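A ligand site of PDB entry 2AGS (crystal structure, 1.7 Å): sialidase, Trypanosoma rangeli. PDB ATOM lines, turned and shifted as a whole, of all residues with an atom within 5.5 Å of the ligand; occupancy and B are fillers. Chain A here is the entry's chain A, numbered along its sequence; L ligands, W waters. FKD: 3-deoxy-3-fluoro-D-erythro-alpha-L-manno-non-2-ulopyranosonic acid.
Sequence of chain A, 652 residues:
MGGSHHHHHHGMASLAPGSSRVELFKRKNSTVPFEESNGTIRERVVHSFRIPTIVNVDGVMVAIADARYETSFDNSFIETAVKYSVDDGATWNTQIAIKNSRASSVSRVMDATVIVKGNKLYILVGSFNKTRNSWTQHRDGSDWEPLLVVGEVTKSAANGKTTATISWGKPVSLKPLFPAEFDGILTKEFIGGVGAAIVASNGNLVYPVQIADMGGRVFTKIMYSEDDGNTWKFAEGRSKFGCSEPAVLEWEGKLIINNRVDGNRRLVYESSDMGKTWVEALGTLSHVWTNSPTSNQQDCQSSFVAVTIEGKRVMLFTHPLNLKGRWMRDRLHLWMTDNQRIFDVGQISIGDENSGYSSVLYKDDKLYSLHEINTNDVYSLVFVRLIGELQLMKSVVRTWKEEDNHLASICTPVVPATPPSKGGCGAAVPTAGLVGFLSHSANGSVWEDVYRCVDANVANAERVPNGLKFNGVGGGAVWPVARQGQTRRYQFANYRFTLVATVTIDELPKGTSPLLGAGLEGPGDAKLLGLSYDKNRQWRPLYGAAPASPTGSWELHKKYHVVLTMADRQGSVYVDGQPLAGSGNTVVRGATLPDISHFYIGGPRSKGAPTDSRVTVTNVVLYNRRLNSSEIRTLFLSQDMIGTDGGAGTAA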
ATOM      1  N   ARG A  50      -8.410 -11.620 -17.430  1.00  0.00           N
ATOM      2  CA  ARG A  50      -7.971 -12.447 -18.520  1.00  0.00           C
ATOM      3  C   ARG A  50      -6.680 -11.877 -19.091  1.00  0.00           C
ATOM      4  O   ARG A  50      -6.236 -10.793 -18.727  1.00  0.00           O
ATOM      5  CB  ARG A  50      -9.056 -12.547 -19.623  1.00  0.00           C
ATOM      6  CG  ARG A  50     -10.268 -13.401 -19.213  1.00  0.00           C
ATOM      7  CD  ARG A  50     -10.909 -14.065 -20.431  1.00  0.00           C
ATOM      8  NE  ARG A  50      -9.885 -14.864 -21.101  1.00  0.00           N
ATOM      9  CZ  ARG A  50      -9.903 -15.208 -22.373  1.00  0.00           C
ATOM     10  NH1 ARG A  50      -8.869 -15.872 -22.852  1.00  0.00           N
ATOM     11  NH2 ARG A  50     -10.931 -14.932 -23.166  1.00  0.00           N
ATOM     12  N   ILE A  51      -6.075 -12.653 -19.981  1.00  0.00           N
ATOM     13  CA  ILE A  51      -4.970 -12.184 -20.812  1.00  0.00           C
ATOM     14  C   ILE A  51      -3.768 -11.759 -19.976  1.00  0.00           C
ATOM     15  O   ILE A  51      -3.312 -10.583 -20.063  1.00  0.00           O
ATOM     16  CB  ILE A  51      -5.409 -11.014 -21.754  1.00  0.00           C
ATOM     17  CG1 ILE A  51      -6.867 -11.159 -22.272  1.00  0.00           C
ATOM     18  CG2 ILE A  51      -4.397 -10.876 -22.916  1.00  0.00           C
ATOM     19  CD1 ILE A  51      -7.187 -12.403 -22.978  1.00  0.00           C
ATOM     20  N   ASP A  66      -6.252  -8.071 -18.615  1.00  0.00           N
ATOM     21  CA  ASP A  66      -7.558  -7.432 -18.940  1.00  0.00           C
ATOM     22  C   ASP A  66      -8.335  -7.521 -17.641  1.00  0.00           C
ATOM     23  O   ASP A  66      -8.497  -8.612 -17.121  1.00  0.00           O
ATOM     24  CB  ASP A  66      -8.394  -8.240 -19.897  1.00  0.00           C
ATOM     25  CG  ASP A  66      -8.135  -8.002 -21.362  1.00  0.00           C
ATOM     26  OD1 ASP A  66      -7.099  -7.444 -21.817  1.00  0.00           O
ATOM     27  OD2 ASP A  66      -9.057  -8.430 -22.125  1.00  0.00           O
ATOM     28  N   ARG A  68     -11.971  -7.454 -17.063  1.00  0.00           N
ATOM     29  CA  ARG A  68     -13.204  -7.511 -17.810  1.00  0.00           C
ATOM     30  C   ARG A  68     -14.258  -7.312 -16.727  1.00  0.00           C
ATOM     31  O   ARG A  68     -14.677  -8.256 -16.045  1.00  0.00           O
ATOM     32  CB  ARG A  68     -13.380  -8.824 -18.571  1.00  0.00           C
ATOM     33  CG  ARG A  68     -12.213  -9.071 -19.511  1.00  0.00           C
ATOM     34  CD  ARG A  68     -12.539 -10.086 -20.549  1.00  0.00           C
ATOM     35  NE  ARG A  68     -11.496 -10.113 -21.580  1.00  0.00           N
ATOM     36  CZ  ARG A  68     -11.546 -10.891 -22.644  1.00  0.00           C
ATOM     37  NH1 ARG A  68     -12.544 -11.728 -22.839  1.00  0.00           N
ATOM     38  NH2 ARG A  68     -10.561 -10.854 -23.527  1.00  0.00           N
ATOM     39  N   ASP A  74     -15.412 -10.955 -24.892  1.00  0.00           N
ATOM     40  CA  ASP A  74     -14.325 -10.179 -25.470  1.00  0.00           C
ATOM     41  C   ASP A  74     -14.757  -8.750 -25.723  1.00  0.00           C
ATOM     42  O   ASP A  74     -14.019  -7.804 -25.475  1.00  0.00           O
ATOM     43  CB  ASP A  74     -13.822 -10.829 -26.767  1.00  0.00           C
ATOM     44  CG  ASP A  74     -13.303 -12.270 -26.564  1.00  0.00           C
ATOM     45  OD1 ASP A  74     -13.227 -12.991 -27.601  1.00  0.00           O
ATOM     46  OD2 ASP A  74     -13.008 -12.712 -25.409  1.00  0.00           O
ATOM     47  N   MET A 110      -7.677  -3.752 -24.745  1.00  0.00           N
ATOM     48  CA  MET A 110      -7.639  -5.219 -24.814  1.00  0.00           C
ATOM     49  C   MET A 110      -6.286  -5.798 -25.249  1.00  0.00           C
ATOM     50  O   MET A 110      -5.529  -5.145 -25.976  1.00  0.00           O
ATOM     51  CB  MET A 110      -8.766  -5.691 -25.763  1.00  0.00           C
ATOM     52  CG  MET A 110      -8.780  -5.129 -27.188  1.00  0.00           C
ATOM     53  SD  MET A 110      -7.635  -5.940 -28.302  1.00  0.00           S
ATOM     54  CE  MET A 110      -8.561  -7.408 -28.732  1.00  0.00           C
ATOM     55  N   ASP A 111      -6.009  -7.037 -24.811  1.00  0.00           N
ATOM     56  CA  ASP A 111      -4.971  -7.846 -25.393  1.00  0.00           C
ATOM     57  C   ASP A 111      -3.599  -7.221 -25.318  1.00  0.00           C
ATOM     58  O   ASP A 111      -2.892  -7.128 -26.310  1.00  0.00           O
ATOM     59  CB  ASP A 111      -5.306  -8.306 -26.812  1.00  0.00           C
ATOM     60  CG  ASP A 111      -6.441  -9.321 -26.832  1.00  0.00           C
ATOM     61  OD1 ASP A 111      -7.020  -9.654 -25.764  1.00  0.00           O
ATOM     62  OD2 ASP A 111      -6.754  -9.777 -27.961  1.00  0.00           O
ATOM     63  N   SER A 134     -16.125  -8.954 -32.875  1.00  0.00           N
ATOM     64  CA  SER A 134     -14.705  -8.999 -32.684  1.00  0.00           C
ATOM     65  C   SER A 134     -13.961  -8.302 -33.806  1.00  0.00           C
ATOM     66  O   SER A 134     -14.457  -8.120 -34.924  1.00  0.00           O
ATOM     67  CB  SER A 134     -14.255 -10.428 -32.441  1.00  0.00           C
ATOM     68  OG  SER A 134     -14.695 -10.828 -31.125  1.00  0.00           O
ATOM     69  N   TRP A 135     -12.756  -7.908 -33.465  1.00  0.00           N
ATOM     70  CA  TRP A 135     -11.987  -7.003 -34.281  1.00  0.00           C
ATOM     71  C   TRP A 135     -11.757  -7.496 -35.692  1.00  0.00           C
ATOM     72  O   TRP A 135     -11.761  -6.712 -36.672  1.00  0.00           O
ATOM     73  CB  TRP A 135     -10.692  -6.690 -33.552  1.00  0.00           C
ATOM     74  CG  TRP A 135      -9.687  -7.799 -33.527  1.00  0.00           C
ATOM     75  CD1 TRP A 135      -9.680  -8.948 -32.725  1.00  0.00           C
ATOM     76  CD2 TRP A 135      -8.511  -7.838 -34.299  1.00  0.00           C
ATOM     77  NE1 TRP A 135      -8.554  -9.706 -33.023  1.00  0.00           N
ATOM     78  CE2 TRP A 135      -7.822  -9.040 -33.980  1.00  0.00           C
ATOM     79  CE3 TRP A 135      -7.968  -6.995 -35.258  1.00  0.00           C
ATOM     80  CZ2 TRP A 135      -6.630  -9.400 -34.614  1.00  0.00           C
ATOM     81  CZ3 TRP A 135      -6.780  -7.345 -35.856  1.00  0.00           C
ATOM     82  CH2 TRP A 135      -6.124  -8.520 -35.515  1.00  0.00           C
ATOM     83  N   THR A 136     -11.594  -8.809 -35.836  1.00  0.00           N
ATOM     84  CA  THR A 136     -11.340  -9.336 -37.143  1.00  0.00           C
ATOM     85  C   THR A 136     -12.562  -9.214 -38.027  1.00  0.00           C
ATOM     86  O   THR A 136     -12.428  -9.221 -39.234  1.00  0.00           O
ATOM     87  CB  THR A 136     -10.941 -10.817 -37.056  1.00  0.00           C
ATOM     88  OG1 THR A 136     -11.996 -11.553 -36.459  1.00  0.00           O
ATOM     89  CG2 THR A 136      -9.748 -10.983 -36.145  1.00  0.00           C
ATOM     90  N   ILE A 191      -3.368  -5.436 -33.878  1.00  0.00           N
ATOM     91  CA  ILE A 191      -3.116  -5.362 -32.486  1.00  0.00           C
ATOM     92  C   ILE A 191      -1.803  -6.138 -32.216  1.00  0.00           C
ATOM     93  O   ILE A 191      -1.229  -6.767 -33.135  1.00  0.00           O
ATOM     94  CB  ILE A 191      -4.234  -5.905 -31.683  1.00  0.00           C
ATOM     95  CG1 ILE A 191      -4.522  -7.338 -32.031  1.00  0.00           C
ATOM     96  CG2 ILE A 191      -5.529  -4.994 -31.767  1.00  0.00           C
ATOM     97  CD1 ILE A 191      -5.515  -7.977 -31.048  1.00  0.00           C
ATOM     98  N   GLN A 210      -0.651  -8.753 -34.987  1.00  0.00           N
ATOM     99  CA  GLN A 210      -1.678  -9.434 -35.683  1.00  0.00           C
ATOM    100  C   GLN A 210      -2.335  -8.419 -36.573  1.00  0.00           C
ATOM    101  O   GLN A 210      -2.754  -7.364 -36.076  1.00  0.00           O
ATOM    102  CB  GLN A 210      -2.733  -9.916 -34.679  1.00  0.00           C
ATOM    103  CG  GLN A 210      -2.255 -10.623 -33.497  1.00  0.00           C
ATOM    104  CD  GLN A 210      -3.373 -11.055 -32.605  1.00  0.00           C
ATOM    105  OE1 GLN A 210      -3.535 -10.580 -31.446  1.00  0.00           O
ATOM    106  NE2 GLN A 210      -4.159 -11.977 -33.125  1.00  0.00           N
ATOM    107  N   SER A 244      -2.267 -15.992 -35.931  1.00  0.00           N
ATOM    108  CA  SER A 244      -2.734 -14.972 -35.046  1.00  0.00           C
ATOM    109  C   SER A 244      -1.853 -15.024 -33.784  1.00  0.00           C
ATOM    110  O   SER A 244      -0.961 -15.831 -33.699  1.00  0.00           O
ATOM    111  CB  SER A 244      -4.208 -15.171 -34.684  1.00  0.00           C
ATOM    112  OG  SER A 244      -4.401 -16.407 -34.002  1.00  0.00           O
ATOM    113  N   GLU A 245      -2.113 -14.123 -32.841  1.00  0.00           N
ATOM    114  CA  GLU A 245      -1.440 -14.062 -31.514  1.00  0.00           C
ATOM    115  C   GLU A 245      -0.003 -14.546 -31.544  1.00  0.00           C
ATOM    116  O   GLU A 245       0.410 -15.483 -30.843  1.00  0.00           O
ATOM    117  CB  GLU A 245      -2.270 -14.725 -30.422  1.00  0.00           C
ATOM    118  CG  GLU A 245      -3.492 -13.909 -30.111  1.00  0.00           C
ATOM    119  CD  GLU A 245      -4.415 -14.498 -29.080  1.00  0.00           C
ATOM    120  OE1 GLU A 245      -4.327 -15.689 -28.817  1.00  0.00           O
ATOM    121  OE2 GLU A 245      -5.249 -13.726 -28.543  1.00  0.00           O
ATOM    122  N   ARG A 260      -0.212 -18.552 -32.980  1.00  0.00           N
ATOM    123  CA  ARG A 260      -1.475 -19.199 -32.817  1.00  0.00           C
ATOM    124  C   ARG A 260      -2.062 -19.486 -34.187  1.00  0.00           C
ATOM    125  O   ARG A 260      -1.966 -18.657 -35.087  1.00  0.00           O
ATOM    126  CB  ARG A 260      -2.413 -18.309 -32.028  1.00  0.00           C
ATOM    127  CG  ARG A 260      -3.744 -18.885 -31.778  1.00  0.00           C
ATOM    128  CD  ARG A 260      -4.597 -18.038 -30.879  1.00  0.00           C
ATOM    129  NE  ARG A 260      -5.990 -18.473 -30.983  1.00  0.00           N
ATOM    130  CZ  ARG A 260      -6.993 -18.033 -30.231  1.00  0.00           C
ATOM    131  NH1 ARG A 260      -6.746 -17.226 -29.224  1.00  0.00           N
ATOM    132  NH2 ARG A 260      -8.230 -18.454 -30.445  1.00  0.00           N
ATOM    133  N   ASP A 262      -5.677 -21.080 -35.273  1.00  0.00           N
ATOM    134  CA  ASP A 262      -6.945 -21.767 -34.998  1.00  0.00           C
ATOM    135  C   ASP A 262      -7.162 -22.834 -36.047  1.00  0.00           C
ATOM    136  O   ASP A 262      -7.064 -22.582 -37.265  1.00  0.00           O
ATOM    137  CB  ASP A 262      -8.072 -20.759 -35.041  1.00  0.00           C
ATOM    138  CG  ASP A 262      -7.987 -19.762 -33.904  1.00  0.00           C
ATOM    139  OD1 ASP A 262      -8.243 -18.558 -34.161  1.00  0.00           O
ATOM    140  OD2 ASP A 262      -7.659 -20.181 -32.772  1.00  0.00           O
ATOM    141  N   GLN A 298     -10.216 -24.467 -31.955  1.00  0.00           N
ATOM    142  CA  GLN A 298      -9.731 -23.111 -31.669  1.00  0.00           C
ATOM    143  C   GLN A 298      -8.379 -23.288 -30.904  1.00  0.00           C
ATOM    144  O   GLN A 298      -8.270 -24.109 -30.003  1.00  0.00           O
ATOM    145  CB  GLN A 298     -10.790 -22.508 -30.761  1.00  0.00           C
ATOM    146  CG  GLN A 298     -10.800 -21.152 -30.273  1.00  0.00           C
ATOM    147  CD  GLN A 298     -12.079 -21.015 -29.334  1.00  0.00           C
ATOM    148  OE1 GLN A 298     -12.220 -20.049 -28.628  1.00  0.00           O
ATOM    149  NE2 GLN A 298     -12.968 -22.051 -29.363  1.00  0.00           N
ATOM    150  N   ASP A 299      -7.381 -22.504 -31.269  1.00  0.00           N
ATOM    151  CA  ASP A 299      -6.095 -22.541 -30.596  1.00  0.00           C
ATOM    152  C   ASP A 299      -6.155 -21.558 -29.412  1.00  0.00           C
ATOM    153  O   ASP A 299      -7.217 -21.028 -29.073  1.00  0.00           O
ATOM    154  CB  ASP A 299      -5.011 -22.186 -31.617  1.00  0.00           C
ATOM    155  CG  ASP A 299      -3.593 -22.559 -31.157  1.00  0.00           C
ATOM    156  OD1 ASP A 299      -3.466 -23.152 -30.067  1.00  0.00           O
ATOM    157  OD2 ASP A 299      -2.662 -22.282 -31.940  1.00  0.00           O
ATOM    158  N   ARG A 329      -9.457 -25.427 -22.840  1.00  0.00           N
ATOM    159  CA  ARG A 329      -8.010 -25.176 -22.626  1.00  0.00           C
ATOM    160  C   ARG A 329      -7.512 -25.750 -21.299  1.00  0.00           C
ATOM    161  O   ARG A 329      -6.691 -25.183 -20.609  1.00  0.00           O
ATOM    162  CB  ARG A 329      -7.742 -23.691 -22.748  1.00  0.00           C
ATOM    163  CG  ARG A 329      -7.911 -23.211 -24.148  1.00  0.00           C
ATOM    164  CD  ARG A 329      -8.222 -21.760 -24.181  1.00  0.00           C
ATOM    165  NE  ARG A 329      -8.368 -21.324 -25.583  1.00  0.00           N
ATOM    166  CZ  ARG A 329      -8.812 -20.119 -25.931  1.00  0.00           C
ATOM    167  NH1 ARG A 329      -9.116 -19.236 -25.007  1.00  0.00           N
ATOM    168  NH2 ARG A 329      -8.882 -19.792 -27.202  1.00  0.00           N
ATOM    169  N   TYR A 357      -5.014 -18.622 -21.412  1.00  0.00           N
ATOM    170  CA  TYR A 357      -3.848 -17.840 -21.805  1.00  0.00           C
ATOM    171  C   TYR A 357      -2.901 -17.831 -20.605  1.00  0.00           C
ATOM    172  O   TYR A 357      -3.303 -18.039 -19.439  1.00  0.00           O
ATOM    173  CB  TYR A 357      -4.259 -16.423 -22.145  1.00  0.00           C
ATOM    174  CG  TYR A 357      -4.977 -16.143 -23.453  1.00  0.00           C
ATOM    175  CD1 TYR A 357      -5.779 -17.087 -24.087  1.00  0.00           C
ATOM    176  CD2 TYR A 357      -4.868 -14.891 -24.061  1.00  0.00           C
ATOM    177  CE1 TYR A 357      -6.467 -16.767 -25.317  1.00  0.00           C
ATOM    178  CE2 TYR A 357      -5.541 -14.584 -25.244  1.00  0.00           C
ATOM    179  CZ  TYR A 357      -6.367 -15.512 -25.879  1.00  0.00           C
ATOM    180  OH  TYR A 357      -7.087 -15.212 -27.045  1.00  0.00           O
HETATM  181  C1  FKD L   1      -9.300 -16.221 -26.677  1.00  0.00           C
HETATM  182  F1  FKD L   1     -10.331 -13.814 -25.936  1.00  0.00           F
HETATM  183  C2  FKD L   1      -8.502 -14.974 -27.051  1.00  0.00           C
HETATM  184  C3  FKD L   1      -8.998 -13.840 -26.151  1.00  0.00           C
HETATM  185  C4  FKD L   1      -8.598 -12.498 -26.764  1.00  0.00           C
HETATM  186  O4  FKD L   1      -8.951 -11.444 -25.880  1.00  0.00           O
HETATM  187  C5  FKD L   1      -9.194 -12.348 -28.147  1.00  0.00           C
HETATM  188  O5  FKD L   1      -8.805 -11.101 -28.725  1.00  0.00           O
HETATM  189  C6  FKD L   1      -8.698 -13.531 -28.988  1.00  0.00           C
HETATM  190  O6  FKD L   1      -9.012 -14.777 -28.378  1.00  0.00           O
HETATM  191  C7  FKD L   1      -9.444 -13.551 -30.342  1.00  0.00           C
HETATM  192  O7  FKD L   1     -10.867 -13.707 -30.133  1.00  0.00           O
HETATM  193  C8  FKD L   1      -8.959 -14.711 -31.199  1.00  0.00           C
HETATM  194  O8  FKD L   1      -7.583 -14.514 -31.449  1.00  0.00           O
HETATM  195  C9  FKD L   1      -9.728 -14.740 -32.533  1.00  0.00           C
HETATM  196  O9  FKD L   1      -9.519 -13.519 -33.210  1.00  0.00           O
HETATM  197  O1A FKD L   1      -9.406 -17.063 -27.596  1.00  0.00           O
HETATM  198  O1B FKD L   1      -9.744 -16.414 -25.503  1.00  0.00           O
HETATM  199  O   HOH W   1     -12.328 -17.683 -25.573  1.00  0.00           O
HETATM  200  O   HOH W   2     -12.466 -11.537 -29.792  1.00  0.00           O
HETATM  201  O   HOH W   3     -11.805 -12.459 -33.384  1.00  0.00           O
HETATM  202  O   HOH W   4     -11.017  -9.679 -28.788  1.00  0.00           O
HETATM  203  O   HOH W   5      -6.859 -16.421 -33.217  1.00  0.00           O
HETATM  204  O   HOH W   6      -7.689 -14.155 -35.145  1.00  0.00           O
HETATM  205  O   HOH W   7     -13.604 -13.979 -31.920  1.00  0.00           O
HETATM  206  O   HOH W   8      -6.773 -12.001 -32.149  1.00  0.00           O
HETATM  207  O   HOH W   9     -10.977 -17.874 -29.741  1.00  0.00           O
HETATM  208  O   HOH W  10      -5.482 -11.386 -29.694  1.00  0.00           O
HETATM  209  O   HOH W  11     -12.029 -15.213 -28.134  1.00  0.00           O
HETATM  210  O   HOH W  12     -13.441 -15.108 -25.303  1.00  0.00           O
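N of Asp 111 is in hydrogen-bond range of OD1 of Asp 66, 3.2 Å away.
The backbone carbonyl oxygen of Arg 260 lies within hydrogen-bond range of the backbone NH of Ser 244.
The guanidinium group of Arg 329 is in hydrogen-bond range of the backbone carbonyl oxygen of Asp 299, at 2.8 Å.
The side-chain amide nitrogen of Gln 210 sits close to the backbone NH of Glu 245.
The guanidinium group of Arg 260 lies within hydrogen-bond range of the backbone carbonyl oxygen of Asp 299 (3.1 Å).
The side-chain carboxylate (OD2) of Asp 74 is in salt-bridge range of the guanidinium group (NH2) of Arg 50 (3.8 Å).
The guanidinium group of Arg 260 is in salt-bridge range of the side-chain carboxylate of Asp 262 (3.0 Å).
O of Arg 50 is in hydrogen-bond range of N of Asp 66, at 2.7 Å.
The guanidinium group (NH2) of Arg 329 is in salt-bridge range of an oxygen (O1A) of the ligand (2.8 Å).
The guanidinium group of Arg 260 lies within salt-bridge range of an oxygen (O1A) of the ligand (3.1 Å).
The side-chain carboxylate of Asp 111 sits at hydrogen-bond distance from an oxygen (O5) of the ligand (2.6 Å).
The side-chain hydroxyl (OH) of Tyr 357 is covalently linked to a carbon (C2) of the ligand (1.4 Å).
NH1 of Arg 50 is in salt-bridge range of O1B of the ligand.
NH2 of Arg 68 is in hydrogen-bond range of O4 of the ligand, at 2.9 Å.
OD2 of Asp 74 lies close to F1 of the ligand (2.9 Å).
Merely in contact with the ligand: Glu 245, Ile 51, Met 110, Thr 136 and Trp 135.
Hydrophobic or aromatic side chains that line the ligand: Ile 51, Met 110 and Tyr 357.
Of the 20 residues printed, 12 come within 4 Å of the ligand.
Water W3 lies within hydrogen-bond range of O9 of the ligand and OG1 of Thr 136.
Water W5 lies within hydrogen-bond range of OG of Ser 244 (2.6 Å), O8 of the ligand (2.7 Å), OD1 of Asp 262 (2.7 Å) and NE of Arg 260 (3.2 Å).
Water W2 lies within hydrogen-bond range of OG of Ser 134 (2.7 Å), O7 of the ligand (2.7 Å) and OD1 of Asp 74 (2.7 Å).
Water W11 bridges the side-chain carboxylate (OD1) of Asp 74 and an oxygen (O7) of the ligand.
Water W9 lies within hydrogen-bond range of the side-chain amide oxygen of Gln 298 (2.7 Å), an oxygen (O1A) of the ligand (2.8 Å) and the guanidinium group of Arg 260 (2.9 Å).
Water W12 lies within hydrogen-bond range of OD2 of Asp 74 and NH2 of Arg 50.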
